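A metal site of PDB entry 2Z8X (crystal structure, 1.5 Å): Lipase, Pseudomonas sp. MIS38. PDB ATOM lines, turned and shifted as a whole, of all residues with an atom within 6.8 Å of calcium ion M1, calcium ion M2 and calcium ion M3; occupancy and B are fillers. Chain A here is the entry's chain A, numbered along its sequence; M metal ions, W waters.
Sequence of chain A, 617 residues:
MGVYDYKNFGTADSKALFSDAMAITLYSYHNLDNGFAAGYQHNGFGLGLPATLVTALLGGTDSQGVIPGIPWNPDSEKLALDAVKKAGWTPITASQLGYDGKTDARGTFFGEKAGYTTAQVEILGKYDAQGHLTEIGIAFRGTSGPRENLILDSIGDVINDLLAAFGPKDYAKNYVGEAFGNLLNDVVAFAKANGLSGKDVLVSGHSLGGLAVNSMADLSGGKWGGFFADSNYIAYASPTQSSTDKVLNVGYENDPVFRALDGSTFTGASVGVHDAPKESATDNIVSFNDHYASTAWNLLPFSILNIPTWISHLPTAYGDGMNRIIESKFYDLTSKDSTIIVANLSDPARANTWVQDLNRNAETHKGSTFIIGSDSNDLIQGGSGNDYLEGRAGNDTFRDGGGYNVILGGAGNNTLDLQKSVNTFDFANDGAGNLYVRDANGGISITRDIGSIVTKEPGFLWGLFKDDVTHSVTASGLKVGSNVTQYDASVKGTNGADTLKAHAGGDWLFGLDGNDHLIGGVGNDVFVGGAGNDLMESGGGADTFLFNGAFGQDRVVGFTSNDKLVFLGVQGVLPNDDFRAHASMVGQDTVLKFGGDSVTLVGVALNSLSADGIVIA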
ATOM      1  N   GLY A 493      11.233  14.283  10.349  1.00  0.00           N
ATOM      2  CA  GLY A 493       9.902  14.491  10.876  1.00  0.00           C
ATOM      3  C   GLY A 493       9.916  15.177  12.221  1.00  0.00           C
ATOM      4  O   GLY A 493      10.799  16.006  12.514  1.00  0.00           O
ATOM      5  N   THR A 494       8.914  14.862  13.030  1.00  0.00           N
ATOM      6  CA  THR A 494       8.767  15.391  14.377  1.00  0.00           C
ATOM      7  C   THR A 494       8.481  14.213  15.297  1.00  0.00           C
ATOM      8  O   THR A 494       8.374  13.054  14.839  1.00  0.00           O
ATOM      9  CB  THR A 494       7.575  16.384  14.470  1.00  0.00           C
ATOM     10  OG1 THR A 494       6.331  15.681  14.320  1.00  0.00           O
ATOM     11  CG2 THR A 494       7.681  17.464  13.401  1.00  0.00           C
ATOM     12  N   ASN A 495       8.307  14.463  16.582  1.00  0.00           N
ATOM     13  CA  ASN A 495       7.938  13.368  17.469  1.00  0.00           C
ATOM     14  C   ASN A 495       6.441  13.058  17.503  1.00  0.00           C
ATOM     15  O   ASN A 495       6.002  12.231  18.262  1.00  0.00           O
ATOM     16  CB  ASN A 495       8.493  13.595  18.873  1.00  0.00           C
ATOM     17  CG  ASN A 495       9.983  13.329  18.976  1.00  0.00           C
ATOM     18  OD1 ASN A 495      10.519  12.428  18.359  1.00  0.00           O
ATOM     19  ND2 ASN A 495      10.650  14.120  19.785  1.00  0.00           N
ATOM     20  N   GLY A 496       5.702  13.726  16.637  1.00  0.00           N
ATOM     21  CA  GLY A 496       4.306  13.349  16.365  1.00  0.00           C
ATOM     22  C   GLY A 496       4.202  12.544  15.078  1.00  0.00           C
ATOM     23  O   GLY A 496       5.222  12.171  14.489  1.00  0.00           O
ATOM     24  N   ALA A 497       2.974  12.249  14.645  1.00  0.00           N
ATOM     25  CA  ALA A 497       2.760  11.502  13.400  1.00  0.00           C
ATOM     26  C   ALA A 497       3.005  12.394  12.178  1.00  0.00           C
ATOM     27  O   ALA A 497       2.389  13.459  12.039  1.00  0.00           O
ATOM     28  CB  ALA A 497       1.355  10.921  13.375  1.00  0.00           C
ATOM     29  N   ASP A 498       3.910  11.947  11.311  1.00  0.00           N
ATOM     30  CA  ASP A 498       4.281  12.699  10.103  1.00  0.00           C
ATOM     31  C   ASP A 498       4.090  11.873   8.854  1.00  0.00           C
ATOM     32  O   ASP A 498       4.217  10.653   8.887  1.00  0.00           O
ATOM     33  CB  ASP A 498       5.758  13.095  10.120  1.00  0.00           C
ATOM     34  CG  ASP A 498       6.212  13.649  11.450  1.00  0.00           C
ATOM     35  OD1 ASP A 498       5.715  14.724  11.835  1.00  0.00           O
ATOM     36  OD2 ASP A 498       7.089  13.000  12.085  1.00  0.00           O
ATOM     37  N   LEU A 500       6.258  11.829   5.467  1.00  0.00           N
ATOM     38  CA  LEU A 500       7.500  12.348   4.882  1.00  0.00           C
ATOM     39  C   LEU A 500       7.643  11.754   3.495  1.00  0.00           C
ATOM     40  O   LEU A 500       7.448  10.558   3.304  1.00  0.00           O
ATOM     41  CB  LEU A 500       8.718  11.954   5.730  1.00  0.00           C
ATOM     42  CG  LEU A 500       8.729  12.359   7.201  1.00  0.00           C
ATOM     43  CD1 LEU A 500      10.075  11.964   7.801  1.00  0.00           C
ATOM     44  CD2 LEU A 500       8.460  13.849   7.366  1.00  0.00           C
ATOM     45  N   PHE A 510      13.713  10.308   8.285  1.00  0.00           N
ATOM     46  CA  PHE A 510      13.767  10.131   9.736  1.00  0.00           C
ATOM     47  C   PHE A 510      12.422  10.452  10.374  1.00  0.00           C
ATOM     48  O   PHE A 510      12.093  11.615  10.614  1.00  0.00           O
ATOM     49  CB  PHE A 510      14.840  11.049  10.340  1.00  0.00           C
ATOM     50  CG  PHE A 510      16.236  10.753   9.870  1.00  0.00           C
ATOM     51  CD1 PHE A 510      16.874   9.570  10.235  1.00  0.00           C
ATOM     52  CD2 PHE A 510      16.930  11.689   9.117  1.00  0.00           C
ATOM     53  CE1 PHE A 510      18.178   9.317   9.837  1.00  0.00           C
ATOM     54  CE2 PHE A 510      18.223  11.445   8.716  1.00  0.00           C
ATOM     55  CZ  PHE A 510      18.857  10.252   9.072  1.00  0.00           C
ATOM     56  N   GLY A 511      11.648   9.412  10.681  1.00  0.00           N
ATOM     57  CA  GLY A 511      10.319   9.604  11.226  1.00  0.00           C
ATOM     58  C   GLY A 511      10.314  10.131  12.652  1.00  0.00           C
ATOM     59  O   GLY A 511       9.399  10.833  13.049  1.00  0.00           O
ATOM     60  N   LEU A 512      11.344   9.758  13.416  1.00  0.00           N
ATOM     61  CA  LEU A 512      11.385  10.037  14.860  1.00  0.00           C
ATOM     62  C   LEU A 512      10.171   9.414  15.576  1.00  0.00           C
ATOM     63  O   LEU A 512       9.575   8.448  15.070  1.00  0.00           O
ATOM     64  CB  LEU A 512      11.490  11.545  15.121  1.00  0.00           C
ATOM     65  CG  LEU A 512      12.568  12.314  14.335  1.00  0.00           C
ATOM     66  CD1 LEU A 512      12.497  13.819  14.652  1.00  0.00           C
ATOM     67  CD2 LEU A 512      13.983  11.740  14.567  1.00  0.00           C
ATOM     68  N   ASP A 513       9.783   9.933  16.745  1.00  0.00           N
ATOM     69  CA  ASP A 513       8.676   9.317  17.482  1.00  0.00           C
ATOM     70  C   ASP A 513       7.338   9.472  16.747  1.00  0.00           C
ATOM     71  O   ASP A 513       7.231  10.263  15.808  1.00  0.00           O
ATOM     72  CB  ASP A 513       8.550   9.895  18.898  1.00  0.00           C
ATOM     73  CG  ASP A 513       9.788   9.669  19.765  1.00  0.00           C
ATOM     74  OD1 ASP A 513      10.736   8.943  19.375  1.00  0.00           O
ATOM     75  OD2 ASP A 513       9.805  10.249  20.876  1.00  0.00           O
ATOM     76  N   GLY A 514       6.350   8.699  17.164  1.00  0.00           N
ATOM     77  CA  GLY A 514       5.021   8.763  16.568  1.00  0.00           C
ATOM     78  C   GLY A 514       4.862   7.791  15.414  1.00  0.00           C
ATOM     79  O   GLY A 514       5.847   7.258  14.895  1.00  0.00           O
ATOM     80  N   ASN A 515       3.623   7.573  15.004  1.00  0.00           N
ATOM     81  CA  ASN A 515       3.320   6.623  13.928  1.00  0.00           C
ATOM     82  C   ASN A 515       3.393   7.329  12.592  1.00  0.00           C
ATOM     83  O   ASN A 515       2.469   8.063  12.202  1.00  0.00           O
ATOM     84  CB  ASN A 515       1.932   6.013  14.125  1.00  0.00           C
ATOM     85  CG  ASN A 515       1.773   5.271  15.450  1.00  0.00           C
ATOM     86  OD1 ASN A 515       2.742   4.875  16.094  1.00  0.00           O
ATOM     87  ND2 ASN A 515       0.529   5.083  15.856  1.00  0.00           N
ATOM     88  N   ASP A 516       4.483   7.083  11.871  1.00  0.00           N
ATOM     89  CA  ASP A 516       4.786   7.859  10.686  1.00  0.00           C
ATOM     90  C   ASP A 516       4.473   7.131   9.387  1.00  0.00           C
ATOM     91  O   ASP A 516       4.331   5.915   9.366  1.00  0.00           O
ATOM     92  CB  ASP A 516       6.247   8.300  10.719  1.00  0.00           C
ATOM     93  CG  ASP A 516       6.561   9.089  11.974  1.00  0.00           C
ATOM     94  OD1 ASP A 516       5.866  10.092  12.213  1.00  0.00           O
ATOM     95  OD2 ASP A 516       7.474   8.694  12.715  1.00  0.00           O
ATOM     96  N   LEU A 518       6.074   7.029   5.767  1.00  0.00           N
ATOM     97  CA  LEU A 518       7.279   7.377   5.031  1.00  0.00           C
ATOM     98  C   LEU A 518       7.175   6.928   3.593  1.00  0.00           C
ATOM     99  O   LEU A 518       7.150   5.720   3.320  1.00  0.00           O
ATOM    100  CB  LEU A 518       8.510   6.738   5.704  1.00  0.00           C
ATOM    101  CG  LEU A 518       9.217   7.511   6.822  1.00  0.00           C
ATOM    102  CD1 LEU A 518       8.280   8.220   7.769  1.00  0.00           C
ATOM    103  CD2 LEU A 518      10.224   6.646   7.562  1.00  0.00           C
ATOM    104  N   VAL A 528      14.251   5.328   8.354  1.00  0.00           N
ATOM    105  CA  VAL A 528      14.415   5.162   9.790  1.00  0.00           C
ATOM    106  C   VAL A 528      13.099   5.588  10.442  1.00  0.00           C
ATOM    107  O   VAL A 528      12.908   6.769  10.797  1.00  0.00           O
ATOM    108  CB  VAL A 528      15.611   5.963  10.339  1.00  0.00           C
ATOM    109  CG1 VAL A 528      15.866   5.546  11.782  1.00  0.00           C
ATOM    110  CG2 VAL A 528      16.854   5.699   9.508  1.00  0.00           C
ATOM    111  N   GLY A 529      12.185   4.636  10.588  1.00  0.00           N
ATOM    112  CA  GLY A 529      10.863   4.927  11.144  1.00  0.00           C
ATOM    113  C   GLY A 529      10.959   5.468  12.564  1.00  0.00           C
ATOM    114  O   GLY A 529      10.149   6.316  12.969  1.00  0.00           O
ATOM    115  N   GLY A 530      11.932   4.961  13.305  1.00  0.00           N
ATOM    116  CA  GLY A 530      12.097   5.327  14.721  1.00  0.00           C
ATOM    117  C   GLY A 530      11.036   4.698  15.601  1.00  0.00           C
ATOM    118  O   GLY A 530      10.377   3.721  15.221  1.00  0.00           O
ATOM    119  N   ALA A 531      10.869   5.250  16.801  1.00  0.00           N
ATOM    120  CA  ALA A 531       9.802   4.796  17.686  1.00  0.00           C
ATOM    121  C   ALA A 531       8.445   4.979  17.009  1.00  0.00           C
ATOM    122  O   ALA A 531       8.297   5.772  16.058  1.00  0.00           O
ATOM    123  CB  ALA A 531       9.846   5.549  18.997  1.00  0.00           C
ATOM    124  N   GLY A 532       7.461   4.219  17.489  1.00  0.00           N
ATOM    125  CA  GLY A 532       6.128   4.266  16.934  1.00  0.00           C
ATOM    126  C   GLY A 532       5.965   3.242  15.827  1.00  0.00           C
ATOM    127  O   GLY A 532       6.921   2.569  15.420  1.00  0.00           O
ATOM    128  N   ASN A 533       4.734   3.133  15.340  1.00  0.00           N
ATOM    129  CA  ASN A 533       4.375   2.122  14.351  1.00  0.00           C
ATOM    130  C   ASN A 533       4.347   2.807  13.003  1.00  0.00           C
ATOM    131  O   ASN A 533       3.419   3.564  12.704  1.00  0.00           O
ATOM    132  CB  ASN A 533       3.004   1.515  14.680  1.00  0.00           C
ATOM    133  CG  ASN A 533       2.964   0.853  16.051  1.00  0.00           C
ATOM    134  OD1 ASN A 533       4.005   0.526  16.637  1.00  0.00           O
ATOM    135  ND2 ASN A 533       1.755   0.651  16.565  1.00  0.00           N
ATOM    136  N   ASP A 534       5.372   2.545  12.203  1.00  0.00           N
ATOM    137  CA  ASP A 534       5.584   3.310  10.992  1.00  0.00           C
ATOM    138  C   ASP A 534       5.252   2.512   9.746  1.00  0.00           C
ATOM    139  O   ASP A 534       5.573   1.324   9.659  1.00  0.00           O
ATOM    140  CB  ASP A 534       7.023   3.818  10.943  1.00  0.00           C
ATOM    141  CG  ASP A 534       7.410   4.592  12.184  1.00  0.00           C
ATOM    142  OD1 ASP A 534       6.900   5.716  12.389  1.00  0.00           O
ATOM    143  OD2 ASP A 534       8.215   4.077  12.970  1.00  0.00           O
ATOM    144  N   MET A 536       6.087   2.303   5.867  1.00  0.00           N
ATOM    145  CA  MET A 536       7.219   2.733   5.051  1.00  0.00           C
ATOM    146  C   MET A 536       7.141   2.082   3.671  1.00  0.00           C
ATOM    147  O   MET A 536       7.137   0.856   3.562  1.00  0.00           O
ATOM    148  CB  MET A 536       8.523   2.369   5.774  1.00  0.00           C
ATOM    149  CG  MET A 536       8.582   3.032   7.161  1.00  0.00           C
ATOM    150  SD  MET A 536      10.074   2.680   8.068  1.00  0.00           S
ATOM    151  CE  MET A 536       9.692   1.090   8.762  1.00  0.00           C
ATOM    152  N   PHE A 547      16.312  -0.486  11.705  1.00  0.00           N
ATOM    153  CA  PHE A 547      15.509  -0.707  12.914  1.00  0.00           C
ATOM    154  C   PHE A 547      16.433  -0.783  14.116  1.00  0.00           C
ATOM    155  O   PHE A 547      17.353  -1.589  14.140  1.00  0.00           O
ATOM    156  CB  PHE A 547      14.674  -1.991  12.785  1.00  0.00           C
ATOM    157  CG  PHE A 547      13.835  -2.043  11.550  1.00  0.00           C
ATOM    158  CD1 PHE A 547      12.566  -1.459  11.526  1.00  0.00           C
ATOM    159  CD2 PHE A 547      14.324  -2.641  10.388  1.00  0.00           C
ATOM    160  CE1 PHE A 547      11.802  -1.479  10.372  1.00  0.00           C
ATOM    161  CE2 PHE A 547      13.559  -2.661   9.234  1.00  0.00           C
ATOM    162  CZ  PHE A 547      12.294  -2.081   9.223  1.00  0.00           C
ATOM    163  N   ALA A 550      13.536   0.052  20.672  1.00  0.00           N
ATOM    164  CA  ALA A 550      12.146  -0.375  20.762  1.00  0.00           C
ATOM    165  C   ALA A 550      11.405   0.250  19.576  1.00  0.00           C
ATOM    166  O   ALA A 550      10.730   1.285  19.714  1.00  0.00           O
ATOM    167  CB  ALA A 550      11.539   0.054  22.094  1.00  0.00           C
ATOM    168  N   PHE A 551      11.556  -0.380  18.426  1.00  0.00           N
ATOM    169  CA  PHE A 551      11.194   0.249  17.158  1.00  0.00           C
ATOM    170  C   PHE A 551       9.716   0.140  16.776  1.00  0.00           C
ATOM    171  O   PHE A 551       9.300   0.721  15.778  1.00  0.00           O
ATOM    172  CB  PHE A 551      12.107  -0.216  16.005  1.00  0.00           C
ATOM    173  CG  PHE A 551      12.017  -1.680  15.700  1.00  0.00           C
ATOM    174  CD1 PHE A 551      12.946  -2.574  16.225  1.00  0.00           C
ATOM    175  CD2 PHE A 551      11.019  -2.165  14.866  1.00  0.00           C
ATOM    176  CE1 PHE A 551      12.851  -3.944  15.932  1.00  0.00           C
ATOM    177  CE2 PHE A 551      10.913  -3.522  14.587  1.00  0.00           C
ATOM    178  CZ  PHE A 551      11.839  -4.406  15.115  1.00  0.00           C
ATOM    179  N   GLY A 552       8.930  -0.589  17.578  1.00  0.00           N
ATOM    180  CA  GLY A 552       7.479  -0.635  17.357  1.00  0.00           C
ATOM    181  C   GLY A 552       7.025  -1.710  16.388  1.00  0.00           C
ATOM    182  O   GLY A 552       7.733  -2.696  16.181  1.00  0.00           O
ATOM    183  N   GLN A 553       5.816  -1.524  15.849  1.00  0.00           N
ATOM    184  CA  GLN A 553       5.235  -2.483  14.905  1.00  0.00           C
ATOM    185  C   GLN A 553       5.140  -1.779  13.563  1.00  0.00           C
ATOM    186  O   GLN A 553       4.208  -0.998  13.317  1.00  0.00           O
ATOM    187  CB  GLN A 553       3.843  -2.965  15.334  1.00  0.00           C
ATOM    188  CG  GLN A 553       3.622  -3.025  16.846  1.00  0.00           C
ATOM    189  CD  GLN A 553       4.574  -3.975  17.553  1.00  0.00           C
ATOM    190  OE1 GLN A 553       5.064  -3.669  18.641  1.00  0.00           O
ATOM    191  NE2 GLN A 553       4.813  -5.130  16.953  1.00  0.00           N
ATOM    192  N   ASP A 554       6.102  -2.061  12.697  1.00  0.00           N
ATOM    193  CA  ASP A 554       6.239  -1.358  11.428  1.00  0.00           C
ATOM    194  C   ASP A 554       5.704  -2.208  10.284  1.00  0.00           C
ATOM    195  O   ASP A 554       5.670  -3.412  10.368  1.00  0.00           O
ATOM    196  CB  ASP A 554       7.713  -1.065  11.168  1.00  0.00           C
ATOM    197  CG  ASP A 554       8.328  -0.131  12.187  1.00  0.00           C
ATOM    198  OD1 ASP A 554       7.614   0.764  12.710  1.00  0.00           O
ATOM    199  OD2 ASP A 554       9.545  -0.282  12.418  1.00  0.00           O
ATOM    200  N   SER A 598       8.107  -5.534  15.854  1.00  0.00           N
ATOM    201  CA  SER A 598       7.946  -6.343  14.647  1.00  0.00           C
ATOM    202  C   SER A 598       8.014  -5.527  13.371  1.00  0.00           C
ATOM    203  O   SER A 598       7.707  -4.325  13.369  1.00  0.00           O
ATOM    204  CB  SER A 598       6.616  -7.102  14.661  1.00  0.00           C
ATOM    205  OG  SER A 598       5.518  -6.197  14.563  1.00  0.00           O
HETATM  206 CA    CA M   1       8.093   6.871  14.038  1.00  0.00          CA
HETATM  207 CA    CA M   2       7.247  11.333  13.742  1.00  0.00          CA
HETATM  208 CA    CA M   3       8.942   2.213  14.166  1.00  0.00          CA
HETATM  209  O   HOH W   1      10.881   1.933  12.810  1.00  0.00           O
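Within 4 Å of calcium ion M1: Leu 512, Asp 513, Gly 514, Asp 516, Gly 529, Gly 530, Ala 531 and Asp 534.
Of the 30 residues printed, 7 come within 4 Å of calcium ion M2. Along chain A the residues within 4 Å of calcium ion M2 span positions 494 to 516.
Calcium ion M1 is bound by the backbone carbonyl oxygen of Ala 531, the side-chain carboxylate of Asp 516, the side-chain carboxylate of Asp 534, the backbone carbonyl oxygen of Gly 529, the backbone carbonyl oxygen of Leu 512 and the backbone carbonyl oxygen of Gly 514. Calcium ion M1 has six donor atoms within binding distance. Slightly farther from calcium ion M1 lies the side-chain carboxylate (OD2) of Asp 534 (3.0 Å).
Water W1 lies within hydrogen-bond range of the side-chain carboxylate (OD2) of Asp 554 and the backbone NH (N) of Gly 530.
Calcium ion M2 is bound by O of Gly 511 (2.3 Å). O of Gly 496 is bound to calcium ion M2 (2.3 Å). O of Asp 513 binds calcium ion M2 (2.3 Å). Calcium ion M2 is bound by O of Thr 494 (2.3 Å). The side-chain carboxylate (OD2) of Asp 498 is bound to calcium ion M2 (2.4 Å). OD1 of Asp 516 binds calcium ion M2 (2.4 Å). Calcium ion M2 is bound by the side-chain carboxylate (OD2) of Asp 516 (2.8 Å). Calcium ion M2 has seven donor atoms within binding distance.
O of Val 528 is in hydrogen-bond range of N of Gly 511, 2.9 Å away. The backbone NH of Gly 496 sits at hydrogen-bond distance from the side-chain hydroxyl of Thr 494. The backbone NH of Asp 554 is in hydrogen-bond range of the backbone carbonyl oxygen of Ser 598, 2.9 Å away. The side-chain amide oxygen (OD1) of Asn 495 is in hydrogen-bond range of the backbone NH (N) of Asp 513, at 3.1 Å.
Calcium ion M3 is bound by the backbone carbonyl oxygen (O) of Phe 551 (2.2 Å). Calcium ion M3 is bound by OD2 of Asp 534 (2.3 Å). The backbone carbonyl oxygen (O) of Gly 530 is bound to calcium ion M3, 2.3 Å away. Water W1 binds calcium ion M3, at 2.4 Å. Calcium ion M3 is bound by O of Gly 532 (2.4 Å). Calcium ion M3 is bound by OD1 of Asp 554, at 2.4 Å. Slightly farther from calcium ion M3 lies the side-chain carboxylate (OD2) of Asp 554 (3.1 Å).
The nearest printed residue that does not touch calcium ion M3 is Gly 529 (4.2 Å).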
